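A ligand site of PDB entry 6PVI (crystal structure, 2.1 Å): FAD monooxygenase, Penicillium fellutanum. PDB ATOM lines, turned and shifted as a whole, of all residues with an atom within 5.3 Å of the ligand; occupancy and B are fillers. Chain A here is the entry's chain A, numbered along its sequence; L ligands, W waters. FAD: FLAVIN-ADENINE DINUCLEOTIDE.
N of Asp 316 lies within hydrogen-bond range of O1P of the ligand. The backbone NH (N) of Lys 38 is in hydrogen-bond range of a nitrogen (N3A) of the ligand, at 3.3 Å. The backbone NH (N) of Val 18 sits at hydrogen-bond distance from an oxygen (O2P) of the ligand, 2.9 Å away. OE1 of Glu 37 is in hydrogen-bond range of O3B of the ligand (2.8 Å). NH2 of Arg 109 is in salt-bridge range of O2A of the ligand (3.0 Å). The backbone NH (N) of Asp 47 is in hydrogen-bond range of an oxygen (O4) of the ligand, 2.6 Å away. O2P of the ligand lies within hydrogen-bond range of N of Ile 17, 3.1 Å away. N6A of the ligand is in hydrogen-bond range of O of Val 133, 2.9 Å away. The side-chain hydroxyl (OG) of Ser 39 lies within hydrogen-bond range of an oxygen (O2B) of the ligand, at 3.5 Å. An oxygen (O3') of the ligand sits at hydrogen-bond distance from the side-chain carboxylate (OD2) of Asp 316 (2.6 Å). The backbone NH (N) of Val 133 is in hydrogen-bond range of a nitrogen (N1A) of the ligand (3.2 Å).
Water W2 lies within hydrogen-bond range of an oxygen (O3B) of the ligand (2.6 Å), the guanidinium group of Arg 109 (3.1 Å) and the backbone carbonyl oxygen of Leu 15 (3.1 Å). Water W1 lies within hydrogen-bond range of O2P of the ligand, N of Gly 19, O of Ser 165 and N of Gly 16. Water W4 lies within hydrogen-bond range of OD2 of Asp 316 (2.4 Å), O1A of the ligand (3.0 Å) and N of Val 168 (3.3 Å).
N of Asp 166 lies within hydrogen-bond range of O of Val 13, at 3.2 Å. The side-chain carboxylate (OD2) of Asp 47 lies within salt-bridge range of the guanidinium group (NE) of Arg 192, 3.1 Å away. The side-chain carboxylate (OE2) of Glu 37 is in hydrogen-bond range of the side-chain hydroxyl (OG) of Ser 39 (2.6 Å). The backbone carbonyl oxygen of Phe 36 lies within hydrogen-bond range of the backbone NH of Gly 14 (2.9 Å). N of Ser 165 sits at hydrogen-bond distance from O of Val 13. N of Val 131 sits at hydrogen-bond distance from O of Glu 37, at 2.9 Å. O of Asp 47 is in hydrogen-bond range of N of Arg 109, 2.8 Å away. O of Gly 167 lies close to N of Ala 317 (3.2 Å).
A nitrogen (N3) of the ligand lies close to the guanidinium group (NH1) of Arg 192 (3.2 Å). CG1 of Val 13 touches N1A of the ligand, at 3.6 Å. Gly 14 touches the ligand (CA to O4B, 3.2 Å). Gly 16 touches the ligand (CA to O5B, 3.4 Å). Phe 36 touches the ligand (O to C2A, 3.9 Å). Ile 45 touches the ligand. CA of Gly 46 touches O4 of the ligand (3.4 Å). Cys 48 touches the ligand (O to N3, 3.7 Å). Ile 49 touches the ligand. Val 131 touches the ligand (O to C2A, 3.6 Å). Glu 132 touches the ligand (CA to N1A, 3.9 Å). Ser 165 touches the ligand. Asp 166 touches the ligand. Gly 167 touches the ligand. Trp 256 touches the ligand (CZ2 to C10, 3.3 Å). Gly 315 touches the ligand. Pro 323 touches the ligand. Ala 329 touches the ligand (CB to O4', 3.3 Å). Hydrophobic or aromatic side chains within 4 Å of the ligand: Val 13, Ile 17, Val 18, Ile 45, Ile 49, Val 133, Trp 256, Pro 323 and Ala 329. Within 4 Å of the ligand: Val 13, Gly 14, Gly 16, Ile 17, Val 18, Phe 36, Glu 37, Lys 38, Ser 39, Ile 45, Gly 46, Asp 47, Cys 48, Ile 49, Arg 109, Val 131, Glu 132, Val 133, Ser 165, Asp 166, Gly 167, Arg 192, Trp 256, Gly 315, Asp 316, Pro 323 and Ala 329.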
ATOM      1  N   VAL A  13      33.903 -18.869 -21.476  1.00  0.00           N
ATOM      2  CA  VAL A  13      33.492 -19.114 -22.867  1.00  0.00           C
ATOM      3  C   VAL A  13      32.366 -18.133 -23.200  1.00  0.00           C
ATOM      4  O   VAL A  13      31.294 -18.207 -22.594  1.00  0.00           O
ATOM      5  CB  VAL A  13      33.014 -20.550 -23.090  1.00  0.00           C
ATOM      6  CG1 VAL A  13      32.672 -20.809 -24.565  1.00  0.00           C
ATOM      7  CG2 VAL A  13      34.034 -21.533 -22.573  1.00  0.00           C
ATOM      8  N   GLY A  14      32.609 -17.246 -24.152  1.00  0.00           N
ATOM      9  CA  GLY A  14      31.611 -16.243 -24.506  1.00  0.00           C
ATOM     10  C   GLY A  14      31.877 -14.913 -23.831  1.00  0.00           C
ATOM     11  O   GLY A  14      31.832 -14.812 -22.593  1.00  0.00           O
ATOM     12  N   LEU A  15      32.186 -13.882 -24.620  1.00  0.00           N
ATOM     13  CA  LEU A  15      32.375 -12.526 -24.092  1.00  0.00           C
ATOM     14  C   LEU A  15      31.273 -11.565 -24.555  1.00  0.00           C
ATOM     15  O   LEU A  15      31.536 -10.539 -25.197  1.00  0.00           O
ATOM     16  CB  LEU A  15      33.761 -12.007 -24.478  1.00  0.00           C
ATOM     17  CG  LEU A  15      34.878 -12.711 -23.696  1.00  0.00           C
ATOM     18  CD1 LEU A  15      36.260 -12.360 -24.223  1.00  0.00           C
ATOM     19  CD2 LEU A  15      34.745 -12.433 -22.155  1.00  0.00           C
ATOM     20  N   GLY A  16      30.032 -11.908 -24.260  1.00  0.00           N
ATOM     21  CA  GLY A  16      28.955 -10.932 -24.262  1.00  0.00           C
ATOM     22  C   GLY A  16      29.027 -10.081 -23.015  1.00  0.00           C
ATOM     23  O   GLY A  16      30.095  -9.916 -22.417  1.00  0.00           O
ATOM     24  N   ILE A  17      27.890  -9.559 -22.584  1.00  0.00           N
ATOM     25  CA  ILE A  17      27.860  -8.732 -21.377  1.00  0.00           C
ATOM     26  C   ILE A  17      28.222  -9.568 -20.152  1.00  0.00           C
ATOM     27  O   ILE A  17      29.040  -9.168 -19.314  1.00  0.00           O
ATOM     28  CB  ILE A  17      26.490  -8.070 -21.215  1.00  0.00           C
ATOM     29  CG1 ILE A  17      26.266  -7.033 -22.317  1.00  0.00           C
ATOM     30  CG2 ILE A  17      26.337  -7.487 -19.815  1.00  0.00           C
ATOM     31  CD1 ILE A  17      24.905  -6.370 -22.263  1.00  0.00           C
ATOM     32  N   VAL A  18      27.605 -10.745 -20.000  1.00  0.00           N
ATOM     33  CA  VAL A  18      27.805 -11.503 -18.779  1.00  0.00           C
ATOM     34  C   VAL A  18      29.204 -12.085 -18.727  1.00  0.00           C
ATOM     35  O   VAL A  18      29.843 -12.107 -17.679  1.00  0.00           O
ATOM     36  CB  VAL A  18      26.725 -12.597 -18.661  1.00  0.00           C
ATOM     37  CG1 VAL A  18      26.911 -13.398 -17.396  1.00  0.00           C
ATOM     38  CG2 VAL A  18      25.367 -11.949 -18.624  1.00  0.00           C
ATOM     39  N   GLY A  19      29.719 -12.531 -19.880  1.00  0.00           N
ATOM     40  CA  GLY A  19      31.074 -13.070 -19.913  1.00  0.00           C
ATOM     41  C   GLY A  19      32.118 -12.034 -19.569  1.00  0.00           C
ATOM     42  O   GLY A  19      33.083 -12.329 -18.865  1.00  0.00           O
ATOM     43  N   PHE A  36      37.456 -16.602 -24.021  1.00  0.00           N
ATOM     44  CA  PHE A  36      37.416 -16.951 -25.420  1.00  0.00           C
ATOM     45  C   PHE A  36      36.125 -16.427 -26.009  1.00  0.00           C
ATOM     46  O   PHE A  36      35.099 -16.392 -25.334  1.00  0.00           O
ATOM     47  CB  PHE A  36      37.510 -18.453 -25.628  1.00  0.00           C
ATOM     48  CG  PHE A  36      38.817 -19.046 -25.194  1.00  0.00           C
ATOM     49  CD1 PHE A  36      39.002 -19.434 -23.878  1.00  0.00           C
ATOM     50  CD2 PHE A  36      39.850 -19.211 -26.097  1.00  0.00           C
ATOM     51  CE1 PHE A  36      40.204 -19.975 -23.480  1.00  0.00           C
ATOM     52  CE2 PHE A  36      41.049 -19.743 -25.695  1.00  0.00           C
ATOM     53  CZ  PHE A  36      41.232 -20.128 -24.389  1.00  0.00           C
ATOM     54  N   GLU A  37      36.206 -15.990 -27.259  1.00  0.00           N
ATOM     55  CA  GLU A  37      35.071 -15.443 -27.993  1.00  0.00           C
ATOM     56  C   GLU A  37      35.268 -15.763 -29.465  1.00  0.00           C
ATOM     57  O   GLU A  37      36.373 -15.606 -30.008  1.00  0.00           O
ATOM     58  CB  GLU A  37      34.967 -13.938 -27.771  1.00  0.00           C
ATOM     59  CG  GLU A  37      34.054 -13.248 -28.764  1.00  0.00           C
ATOM     60  CD  GLU A  37      32.639 -13.789 -28.711  1.00  0.00           C
ATOM     61  OE1 GLU A  37      32.061 -13.813 -27.594  1.00  0.00           O
ATOM     62  OE2 GLU A  37      32.120 -14.179 -29.783  1.00  0.00           O
ATOM     63  N   LYS A  38      34.226 -16.256 -30.113  1.00  0.00           N
ATOM     64  CA  LYS A  38      34.375 -16.693 -31.496  1.00  0.00           C
ATOM     65  C   LYS A  38      34.194 -15.560 -32.500  1.00  0.00           C
ATOM     66  O   LYS A  38      34.590 -15.704 -33.656  1.00  0.00           O
ATOM     67  CB  LYS A  38      33.378 -17.801 -31.820  1.00  0.00           C
ATOM     68  CG  LYS A  38      31.927 -17.399 -31.619  1.00  0.00           C
ATOM     69  CD  LYS A  38      30.985 -18.524 -31.972  1.00  0.00           C
ATOM     70  CE  LYS A  38      29.541 -18.092 -31.816  1.00  0.00           C
ATOM     71  NZ  LYS A  38      28.611 -19.241 -31.931  1.00  0.00           N
ATOM     72  N   SER A  39      33.633 -14.438 -32.081  1.00  0.00           N
ATOM     73  CA  SER A  39      33.219 -13.409 -33.015  1.00  0.00           C
ATOM     74  C   SER A  39      33.873 -12.083 -32.673  1.00  0.00           C
ATOM     75  O   SER A  39      34.339 -11.871 -31.552  1.00  0.00           O
ATOM     76  CB  SER A  39      31.697 -13.247 -33.018  1.00  0.00           C
ATOM     77  OG  SER A  39      31.251 -12.727 -31.780  1.00  0.00           O
ATOM     78  N   ILE A  41      33.597  -8.806 -31.373  1.00  0.00           N
ATOM     79  CA  ILE A  41      32.594  -8.216 -30.485  1.00  0.00           C
ATOM     80  C   ILE A  41      32.673  -6.708 -30.421  1.00  0.00           C
ATOM     81  O   ILE A  41      31.750  -6.087 -29.863  1.00  0.00           O
ATOM     82  CB  ILE A  41      32.691  -8.783 -29.060  1.00  0.00           C
ATOM     83  CG1 ILE A  41      34.093  -8.547 -28.489  1.00  0.00           C
ATOM     84  CG2 ILE A  41      32.270 -10.256 -29.060  1.00  0.00           C
ATOM     85  CD1 ILE A  41      34.235  -8.774 -26.992  1.00  0.00           C
ATOM     86  N   ILE A  45      26.433  -3.498 -33.411  1.00  0.00           N
ATOM     87  CA  ILE A  45      25.296  -4.341 -33.746  1.00  0.00           C
ATOM     88  C   ILE A  45      24.345  -4.244 -32.582  1.00  0.00           C
ATOM     89  O   ILE A  45      24.761  -3.972 -31.452  1.00  0.00           O
ATOM     90  CB  ILE A  45      25.759  -5.799 -34.030  1.00  0.00           C
ATOM     91  CG1 ILE A  45      24.567  -6.728 -34.241  1.00  0.00           C
ATOM     92  CG2 ILE A  45      26.628  -6.303 -32.890  1.00  0.00           C
ATOM     93  CD1 ILE A  45      24.982  -8.097 -34.701  1.00  0.00           C
ATOM     94  N   GLY A  46      23.054  -4.425 -32.846  1.00  0.00           N
ATOM     95  CA  GLY A  46      22.052  -4.312 -31.816  1.00  0.00           C
ATOM     96  C   GLY A  46      21.715  -2.869 -31.490  1.00  0.00           C
ATOM     97  O   GLY A  46      22.160  -1.915 -32.130  1.00  0.00           O
ATOM     98  N   ASP A  47      20.915  -2.720 -30.438  1.00  0.00           N
ATOM     99  CA  ASP A  47      20.485  -1.405 -29.993  1.00  0.00           C
ATOM    100  C   ASP A  47      20.893  -1.196 -28.538  1.00  0.00           C
ATOM    101  O   ASP A  47      22.034  -1.463 -28.175  1.00  0.00           O
ATOM    102  CB  ASP A  47      18.977  -1.214 -30.172  1.00  0.00           C
ATOM    103  CG  ASP A  47      18.174  -2.451 -29.775  1.00  0.00           C
ATOM    104  OD1 ASP A  47      17.914  -3.313 -30.650  1.00  0.00           O
ATOM    105  OD2 ASP A  47      17.815  -2.569 -28.574  1.00  0.00           O
ATOM    106  N   CYS A  48      19.962  -0.774 -27.679  1.00  0.00           N
ATOM    107  CA  CYS A  48      20.306  -0.311 -26.352  1.00  0.00           C
ATOM    108  C   CYS A  48      20.051  -1.386 -25.298  1.00  0.00           C
ATOM    109  O   CYS A  48      19.083  -2.146 -25.384  1.00  0.00           O
ATOM    110  CB  CYS A  48      19.525   0.949 -25.990  1.00  0.00           C
ATOM    111  SG  CYS A  48      20.155   2.437 -26.837  1.00  0.00           S
ATOM    112  N   ILE A  49      20.950  -1.418 -24.321  1.00  0.00           N
ATOM    113  CA  ILE A  49      20.837  -2.231 -23.125  1.00  0.00           C
ATOM    114  C   ILE A  49      20.574  -1.287 -21.958  1.00  0.00           C
ATOM    115  O   ILE A  49      21.221  -0.242 -21.837  1.00  0.00           O
ATOM    116  CB  ILE A  49      22.136  -3.033 -22.898  1.00  0.00           C
ATOM    117  CG1 ILE A  49      22.246  -4.169 -23.913  1.00  0.00           C
ATOM    118  CG2 ILE A  49      22.224  -3.576 -21.484  1.00  0.00           C
ATOM    119  CD1 ILE A  49      21.518  -5.430 -23.486  1.00  0.00           C
ATOM    120  N   ARG A 109      24.420  -1.413 -26.794  1.00  0.00           N
ATOM    121  CA  ARG A 109      25.165  -2.587 -26.356  1.00  0.00           C
ATOM    122  C   ARG A 109      26.611  -2.504 -26.804  1.00  0.00           C
ATOM    123  O   ARG A 109      27.515  -2.812 -26.026  1.00  0.00           O
ATOM    124  CB  ARG A 109      24.502  -3.852 -26.891  1.00  0.00           C
ATOM    125  CG  ARG A 109      25.082  -5.151 -26.308  1.00  0.00           C
ATOM    126  CD  ARG A 109      24.448  -6.372 -26.931  1.00  0.00           C
ATOM    127  NE  ARG A 109      25.083  -7.603 -26.510  1.00  0.00           N
ATOM    128  CZ  ARG A 109      26.146  -8.148 -27.105  1.00  0.00           C
ATOM    129  NH1 ARG A 109      26.663  -7.560 -28.173  1.00  0.00           N
ATOM    130  NH2 ARG A 109      26.671  -9.290 -26.652  1.00  0.00           N
ATOM    131  N   VAL A 131      37.897 -17.477 -31.671  1.00  0.00           N
ATOM    132  CA  VAL A 131      38.119 -18.838 -31.160  1.00  0.00           C
ATOM    133  C   VAL A 131      36.791 -19.418 -30.720  1.00  0.00           C
ATOM    134  O   VAL A 131      36.206 -18.974 -29.725  1.00  0.00           O
ATOM    135  CB  VAL A 131      39.129 -18.856 -29.998  1.00  0.00           C
ATOM    136  CG1 VAL A 131      39.231 -20.278 -29.416  1.00  0.00           C
ATOM    137  CG2 VAL A 131      40.492 -18.390 -30.461  1.00  0.00           C
ATOM    138  N   GLU A 132      36.306 -20.414 -31.442  1.00  0.00           N
ATOM    139  CA  GLU A 132      35.138 -21.162 -30.996  1.00  0.00           C
ATOM    140  C   GLU A 132      35.595 -22.245 -30.035  1.00  0.00           C
ATOM    141  O   GLU A 132      36.549 -22.968 -30.310  1.00  0.00           O
ATOM    142  CB  GLU A 132      34.391 -21.764 -32.174  1.00  0.00           C
ATOM    143  CG  GLU A 132      33.086 -22.479 -31.827  1.00  0.00           C
ATOM    144  CD  GLU A 132      32.287 -22.908 -33.056  1.00  0.00           C
ATOM    145  OE1 GLU A 132      32.601 -22.426 -34.169  1.00  0.00           O
ATOM    146  OE2 GLU A 132      31.349 -23.716 -32.916  1.00  0.00           O
ATOM    147  N   VAL A 133      34.917 -22.349 -28.900  1.00  0.00           N
ATOM    148  CA  VAL A 133      35.250 -23.325 -27.876  1.00  0.00           C
ATOM    149  C   VAL A 133      34.212 -24.427 -27.878  1.00  0.00           C
ATOM    150  O   VAL A 133      33.009 -24.154 -28.021  1.00  0.00           O
ATOM    151  CB  VAL A 133      35.337 -22.640 -26.506  1.00  0.00           C
ATOM    152  CG1 VAL A 133      35.409 -23.660 -25.386  1.00  0.00           C
ATOM    153  CG2 VAL A 133      36.541 -21.758 -26.506  1.00  0.00           C
ATOM    154  N   CYS A 134      34.668 -25.659 -27.752  1.00  0.00           N
ATOM    155  CA  CYS A 134      33.770 -26.797 -27.731  1.00  0.00           C
ATOM    156  C   CYS A 134      34.291 -27.841 -26.738  1.00  0.00           C
ATOM    157  O   CYS A 134      35.295 -27.641 -26.050  1.00  0.00           O
ATOM    158  CB  CYS A 134      33.609 -27.391 -29.131  1.00  0.00           C
ATOM    159  SG  CYS A 134      35.146 -28.002 -29.839  1.00  0.00           S
ATOM    160  N   SER A 165      29.388 -18.592 -20.576  1.00  0.00           N
ATOM    161  CA  SER A 165      28.593 -17.397 -20.824  1.00  0.00           C
ATOM    162  C   SER A 165      28.418 -17.194 -22.311  1.00  0.00           C
ATOM    163  O   SER A 165      28.551 -16.079 -22.819  1.00  0.00           O
ATOM    164  CB  SER A 165      29.249 -16.178 -20.206  1.00  0.00           C
ATOM    165  OG  SER A 165      30.641 -16.234 -20.397  1.00  0.00           O
ATOM    166  N   ASP A 166      28.174 -18.280 -23.028  1.00  0.00           N
ATOM    167  CA  ASP A 166      28.005 -18.247 -24.475  1.00  0.00           C
ATOM    168  C   ASP A 166      26.551 -18.044 -24.899  1.00  0.00           C
ATOM    169  O   ASP A 166      26.192 -18.364 -26.036  1.00  0.00           O
ATOM    170  CB  ASP A 166      28.604 -19.523 -25.094  1.00  0.00           C
ATOM    171  CG  ASP A 166      28.129 -20.798 -24.425  1.00  0.00           C
ATOM    172  OD1 ASP A 166      27.811 -20.777 -23.209  1.00  0.00           O
ATOM    173  OD2 ASP A 166      28.098 -21.847 -25.112  1.00  0.00           O
ATOM    174  N   GLY A 167      25.699 -17.498 -24.016  1.00  0.00           N
ATOM    175  CA  GLY A 167      24.415 -16.939 -24.434  1.00  0.00           C
ATOM    176  C   GLY A 167      23.272 -17.925 -24.665  1.00  0.00           C
ATOM    177  O   GLY A 167      23.283 -19.084 -24.224  1.00  0.00           O
ATOM    178  N   VAL A 168      22.261 -17.429 -25.378  1.00  0.00           N
ATOM    179  CA  VAL A 168      21.009 -18.169 -25.492  1.00  0.00           C
ATOM    180  C   VAL A 168      21.178 -19.409 -26.371  1.00  0.00           C
ATOM    181  O   VAL A 168      20.460 -20.399 -26.201  1.00  0.00           O
ATOM    182  CB  VAL A 168      19.880 -17.229 -25.978  1.00  0.00           C
ATOM    183  CG1 VAL A 168      20.235 -16.558 -27.317  1.00  0.00           C
ATOM    184  CG2 VAL A 168      18.560 -17.988 -26.094  1.00  0.00           C
ATOM    185  N   ARG A 192      12.996  -3.674 -33.103  1.00  0.00           N
ATOM    186  CA  ARG A 192      13.811  -2.831 -32.236  1.00  0.00           C
ATOM    187  C   ARG A 192      15.036  -2.361 -32.980  1.00  0.00           C
ATOM    188  O   ARG A 192      15.580  -3.081 -33.811  1.00  0.00           O
ATOM    189  CB  ARG A 192      14.224  -3.580 -30.971  1.00  0.00           C
ATOM    190  CG  ARG A 192      14.602  -4.990 -31.210  1.00  0.00           C
ATOM    191  CD  ARG A 192      14.877  -5.622 -29.888  1.00  0.00           C
ATOM    192  NE  ARG A 192      15.621  -4.676 -29.078  1.00  0.00           N
ATOM    193  CZ  ARG A 192      16.054  -4.948 -27.853  1.00  0.00           C
ATOM    194  NH1 ARG A 192      16.734  -4.040 -27.161  1.00  0.00           N
ATOM    195  NH2 ARG A 192      15.815  -6.126 -27.343  1.00  0.00           N
ATOM    196  N   TRP A 256      20.453 -11.704 -34.132  1.00  0.00           N
ATOM    197  CA  TRP A 256      20.473 -10.245 -34.071  1.00  0.00           C
ATOM    198  C   TRP A 256      20.950  -9.616 -35.385  1.00  0.00           C
ATOM    199  O   TRP A 256      21.305  -8.432 -35.402  1.00  0.00           O
ATOM    200  CB  TRP A 256      21.352  -9.790 -32.905  1.00  0.00           C
ATOM    201  CG  TRP A 256      20.793 -10.113 -31.525  1.00  0.00           C
ATOM    202  CD1 TRP A 256      21.114 -11.192 -30.726  1.00  0.00           C
ATOM    203  CD2 TRP A 256      19.842  -9.340 -30.781  1.00  0.00           C
ATOM    204  NE1 TRP A 256      20.411 -11.134 -29.543  1.00  0.00           N
ATOM    205  CE2 TRP A 256      19.621 -10.006 -29.556  1.00  0.00           C
ATOM    206  CE3 TRP A 256      19.142  -8.147 -31.039  1.00  0.00           C
ATOM    207  CZ2 TRP A 256      18.755  -9.518 -28.593  1.00  0.00           C
ATOM    208  CZ3 TRP A 256      18.278  -7.668 -30.079  1.00  0.00           C
ATOM    209  CH2 TRP A 256      18.083  -8.355 -28.867  1.00  0.00           C
ATOM    210  N   ILE A 314      25.991 -19.362 -16.813  1.00  0.00           N
ATOM    211  CA  ILE A 314      25.504 -18.084 -16.315  1.00  0.00           C
ATOM    212  C   ILE A 314      25.000 -17.247 -17.476  1.00  0.00           C
ATOM    213  O   ILE A 314      25.282 -17.503 -18.656  1.00  0.00           O
ATOM    214  CB  ILE A 314      26.563 -17.300 -15.520  1.00  0.00           C
ATOM    215  CG1 ILE A 314      27.766 -16.934 -16.380  1.00  0.00           C
ATOM    216  CG2 ILE A 314      26.972 -18.033 -14.238  1.00  0.00           C
ATOM    217  CD1 ILE A 314      28.676 -15.868 -15.728  1.00  0.00           C
ATOM    218  N   GLY A 315      24.239 -16.213 -17.118  1.00  0.00           N
ATOM    219  CA  GLY A 315      23.698 -15.299 -18.106  1.00  0.00           C
ATOM    220  C   GLY A 315      22.629 -15.975 -18.959  1.00  0.00           C
ATOM    221  O   GLY A 315      21.887 -16.859 -18.511  1.00  0.00           O
ATOM    222  N   ASP A 316      22.565 -15.550 -20.225  1.00  0.00           N
ATOM    223  CA  ASP A 316      21.571 -16.089 -21.146  1.00  0.00           C
ATOM    224  C   ASP A 316      21.714 -17.588 -21.385  1.00  0.00           C
ATOM    225  O   ASP A 316      20.744 -18.228 -21.806  1.00  0.00           O
ATOM    226  CB  ASP A 316      21.642 -15.323 -22.477  1.00  0.00           C
ATOM    227  CG  ASP A 316      20.887 -14.015 -22.416  1.00  0.00           C
ATOM    228  OD1 ASP A 316      20.563 -13.611 -21.276  1.00  0.00           O
ATOM    229  OD2 ASP A 316      20.588 -13.422 -23.488  1.00  0.00           O
ATOM    230  N   ALA A 317      22.888 -18.173 -21.177  1.00  0.00           N
ATOM    231  CA  ALA A 317      22.974 -19.619 -21.193  1.00  0.00           C
ATOM    232  C   ALA A 317      22.084 -20.221 -20.102  1.00  0.00           C
ATOM    233  O   ALA A 317      21.389 -21.223 -20.339  1.00  0.00           O
ATOM    234  CB  ALA A 317      24.425 -20.064 -21.032  1.00  0.00           C
ATOM    235  N   PRO A 323      14.265  -9.692 -23.964  1.00  0.00           N
ATOM    236  CA  PRO A 323      15.018  -8.437 -23.990  1.00  0.00           C
ATOM    237  C   PRO A 323      14.160  -7.250 -23.581  1.00  0.00           C
ATOM    238  O   PRO A 323      14.708  -6.155 -23.347  1.00  0.00           O
ATOM    239  CB  PRO A 323      15.492  -8.334 -25.436  1.00  0.00           C
ATOM    240  CG  PRO A 323      15.262  -9.689 -26.051  1.00  0.00           C
ATOM    241  CD  PRO A 323      14.104 -10.271 -25.316  1.00  0.00           C
ATOM    242  N   GLY A 328      17.236  -8.180 -17.919  1.00  0.00           N
ATOM    243  CA  GLY A 328      17.995  -9.214 -18.589  1.00  0.00           C
ATOM    244  C   GLY A 328      19.482  -9.153 -18.332  1.00  0.00           C
ATOM    245  O   GLY A 328      20.045 -10.054 -17.699  1.00  0.00           O
ATOM    246  N   ALA A 329      20.155  -8.096 -18.815  1.00  0.00           N
ATOM    247  CA  ALA A 329      21.588  -7.968 -18.567  1.00  0.00           C
ATOM    248  C   ALA A 329      21.906  -7.763 -17.083  1.00  0.00           C
ATOM    249  O   ALA A 329      22.963  -8.194 -16.617  1.00  0.00           O
ATOM    250  CB  ALA A 329      22.165  -6.827 -19.389  1.00  0.00           C
HETATM  251  PA  FAD L   1      25.285 -12.828 -25.171  1.00  0.00           P
HETATM  252  O1A FAD L   1      24.352 -13.329 -26.201  1.00  0.00           O
HETATM  253  O2A FAD L   1      25.296 -11.329 -24.880  1.00  0.00           O
HETATM  254  O5B FAD L   1      26.775 -13.150 -25.548  1.00  0.00           O
HETATM  255  C5B FAD L   1      27.233 -14.500 -25.741  1.00  0.00           C
HETATM  256  C4B FAD L   1      28.523 -14.472 -26.528  1.00  0.00           C
HETATM  257  O4B FAD L   1      29.144 -15.772 -26.536  1.00  0.00           O
HETATM  258  C3B FAD L   1      28.428 -14.022 -27.993  1.00  0.00           C
HETATM  259  O3B FAD L   1      29.461 -13.072 -28.203  1.00  0.00           O
HETATM  260  C2B FAD L   1      28.716 -15.307 -28.784  1.00  0.00           C
HETATM  261  O2B FAD L   1      29.497 -15.109 -29.943  1.00  0.00           O
HETATM  262  C1B FAD L   1      29.670 -16.005 -27.825  1.00  0.00           C
HETATM  263  N9A FAD L   1      29.797 -17.444 -28.030  1.00  0.00           N
HETATM  264  C8A FAD L   1      28.812 -18.375 -28.201  1.00  0.00           C
HETATM  265  N7A FAD L   1      29.253 -19.603 -28.296  1.00  0.00           N
HETATM  266  C5A FAD L   1      30.628 -19.471 -28.185  1.00  0.00           C
HETATM  267  C6A FAD L   1      31.687 -20.404 -28.219  1.00  0.00           C
HETATM  268  N6A FAD L   1      31.526 -21.721 -28.375  1.00  0.00           N
HETATM  269  N1A FAD L   1      32.942 -19.926 -28.085  1.00  0.00           N
HETATM  270  C2A FAD L   1      33.126 -18.615 -27.926  1.00  0.00           C
HETATM  271  N3A FAD L   1      32.213 -17.642 -27.888  1.00  0.00           N
HETATM  272  C4A FAD L   1      30.975 -18.144 -28.034  1.00  0.00           C
HETATM  273  N1  FAD L   1      20.150  -7.564 -25.986  1.00  0.00           N
HETATM  274  C2  FAD L   1      19.425  -6.410 -25.908  1.00  0.00           C
HETATM  275  O2  FAD L   1      18.646  -6.171 -24.981  1.00  0.00           O
HETATM  276  N3  FAD L   1      19.558  -5.459 -26.901  1.00  0.00           N
HETATM  277  C4  FAD L   1      20.374  -5.542 -27.999  1.00  0.00           C
HETATM  278  O4  FAD L   1      20.422  -4.630 -28.814  1.00  0.00           O
HETATM  279  C4X FAD L   1      21.145  -6.769 -28.057  1.00  0.00           C
HETATM  280  N5  FAD L   1      21.954  -6.931 -29.072  1.00  0.00           N
HETATM  281  C5X FAD L   1      22.683  -8.097 -29.145  1.00  0.00           C
HETATM  282  C6  FAD L   1      23.553  -8.273 -30.221  1.00  0.00           C
HETATM  283  C7  FAD L   1      24.326  -9.424 -30.330  1.00  0.00           C
HETATM  284  C7M FAD L   1      25.256  -9.590 -31.501  1.00  0.00           C
HETATM  285  C8  FAD L   1      24.228 -10.419 -29.338  1.00  0.00           C
HETATM  286  C8M FAD L   1      25.051 -11.684 -29.431  1.00  0.00           C
HETATM  287  C9  FAD L   1      23.359 -10.243 -28.262  1.00  0.00           C
HETATM  288  C9A FAD L   1      22.604  -9.086 -28.155  1.00  0.00           C
HETATM  289  N10 FAD L   1      21.725  -8.874 -27.065  1.00  0.00           N
HETATM  290  C10 FAD L   1      20.977  -7.720 -27.003  1.00  0.00           C
HETATM  291  C1' FAD L   1      21.559  -9.900 -26.014  1.00  0.00           C
HETATM  292  C2' FAD L   1      22.131  -9.482 -24.665  1.00  0.00           C
HETATM  293  O2' FAD L   1      23.542  -9.303 -24.761  1.00  0.00           O
HETATM  294  C3' FAD L   1      21.825 -10.572 -23.638  1.00  0.00           C
HETATM  295  O3' FAD L   1      20.420 -10.795 -23.622  1.00  0.00           O
HETATM  296  C4' FAD L   1      22.327 -10.275 -22.228  1.00  0.00           C
HETATM  297  O4' FAD L   1      22.221  -8.873 -21.943  1.00  0.00           O
HETATM  298  C5' FAD L   1      23.745 -10.762 -22.009  1.00  0.00           C
HETATM  299  O5' FAD L   1      23.743 -12.196 -22.120  1.00  0.00           O
HETATM  300  P   FAD L   1      25.089 -13.015 -22.296  1.00  0.00           P
HETATM  301  O1P FAD L   1      24.896 -14.182 -21.330  1.00  0.00           O
HETATM  302  O2P FAD L   1      26.207 -12.118 -22.166  1.00  0.00           O
HETATM  303  O3P FAD L   1      25.019 -13.598 -23.799  1.00  0.00           O
HETATM  304  O   HOH W   1      28.624 -13.373 -22.247  1.00  0.00           O
HETATM  305  O   HOH W   2      29.381 -10.530 -27.491  1.00  0.00           O
HETATM  306  O   HOH W   3      25.398 -16.630 -21.188  1.00  0.00           O
HETATM  307  O   HOH W   4      21.575 -14.207 -25.588  1.00  0.00           O
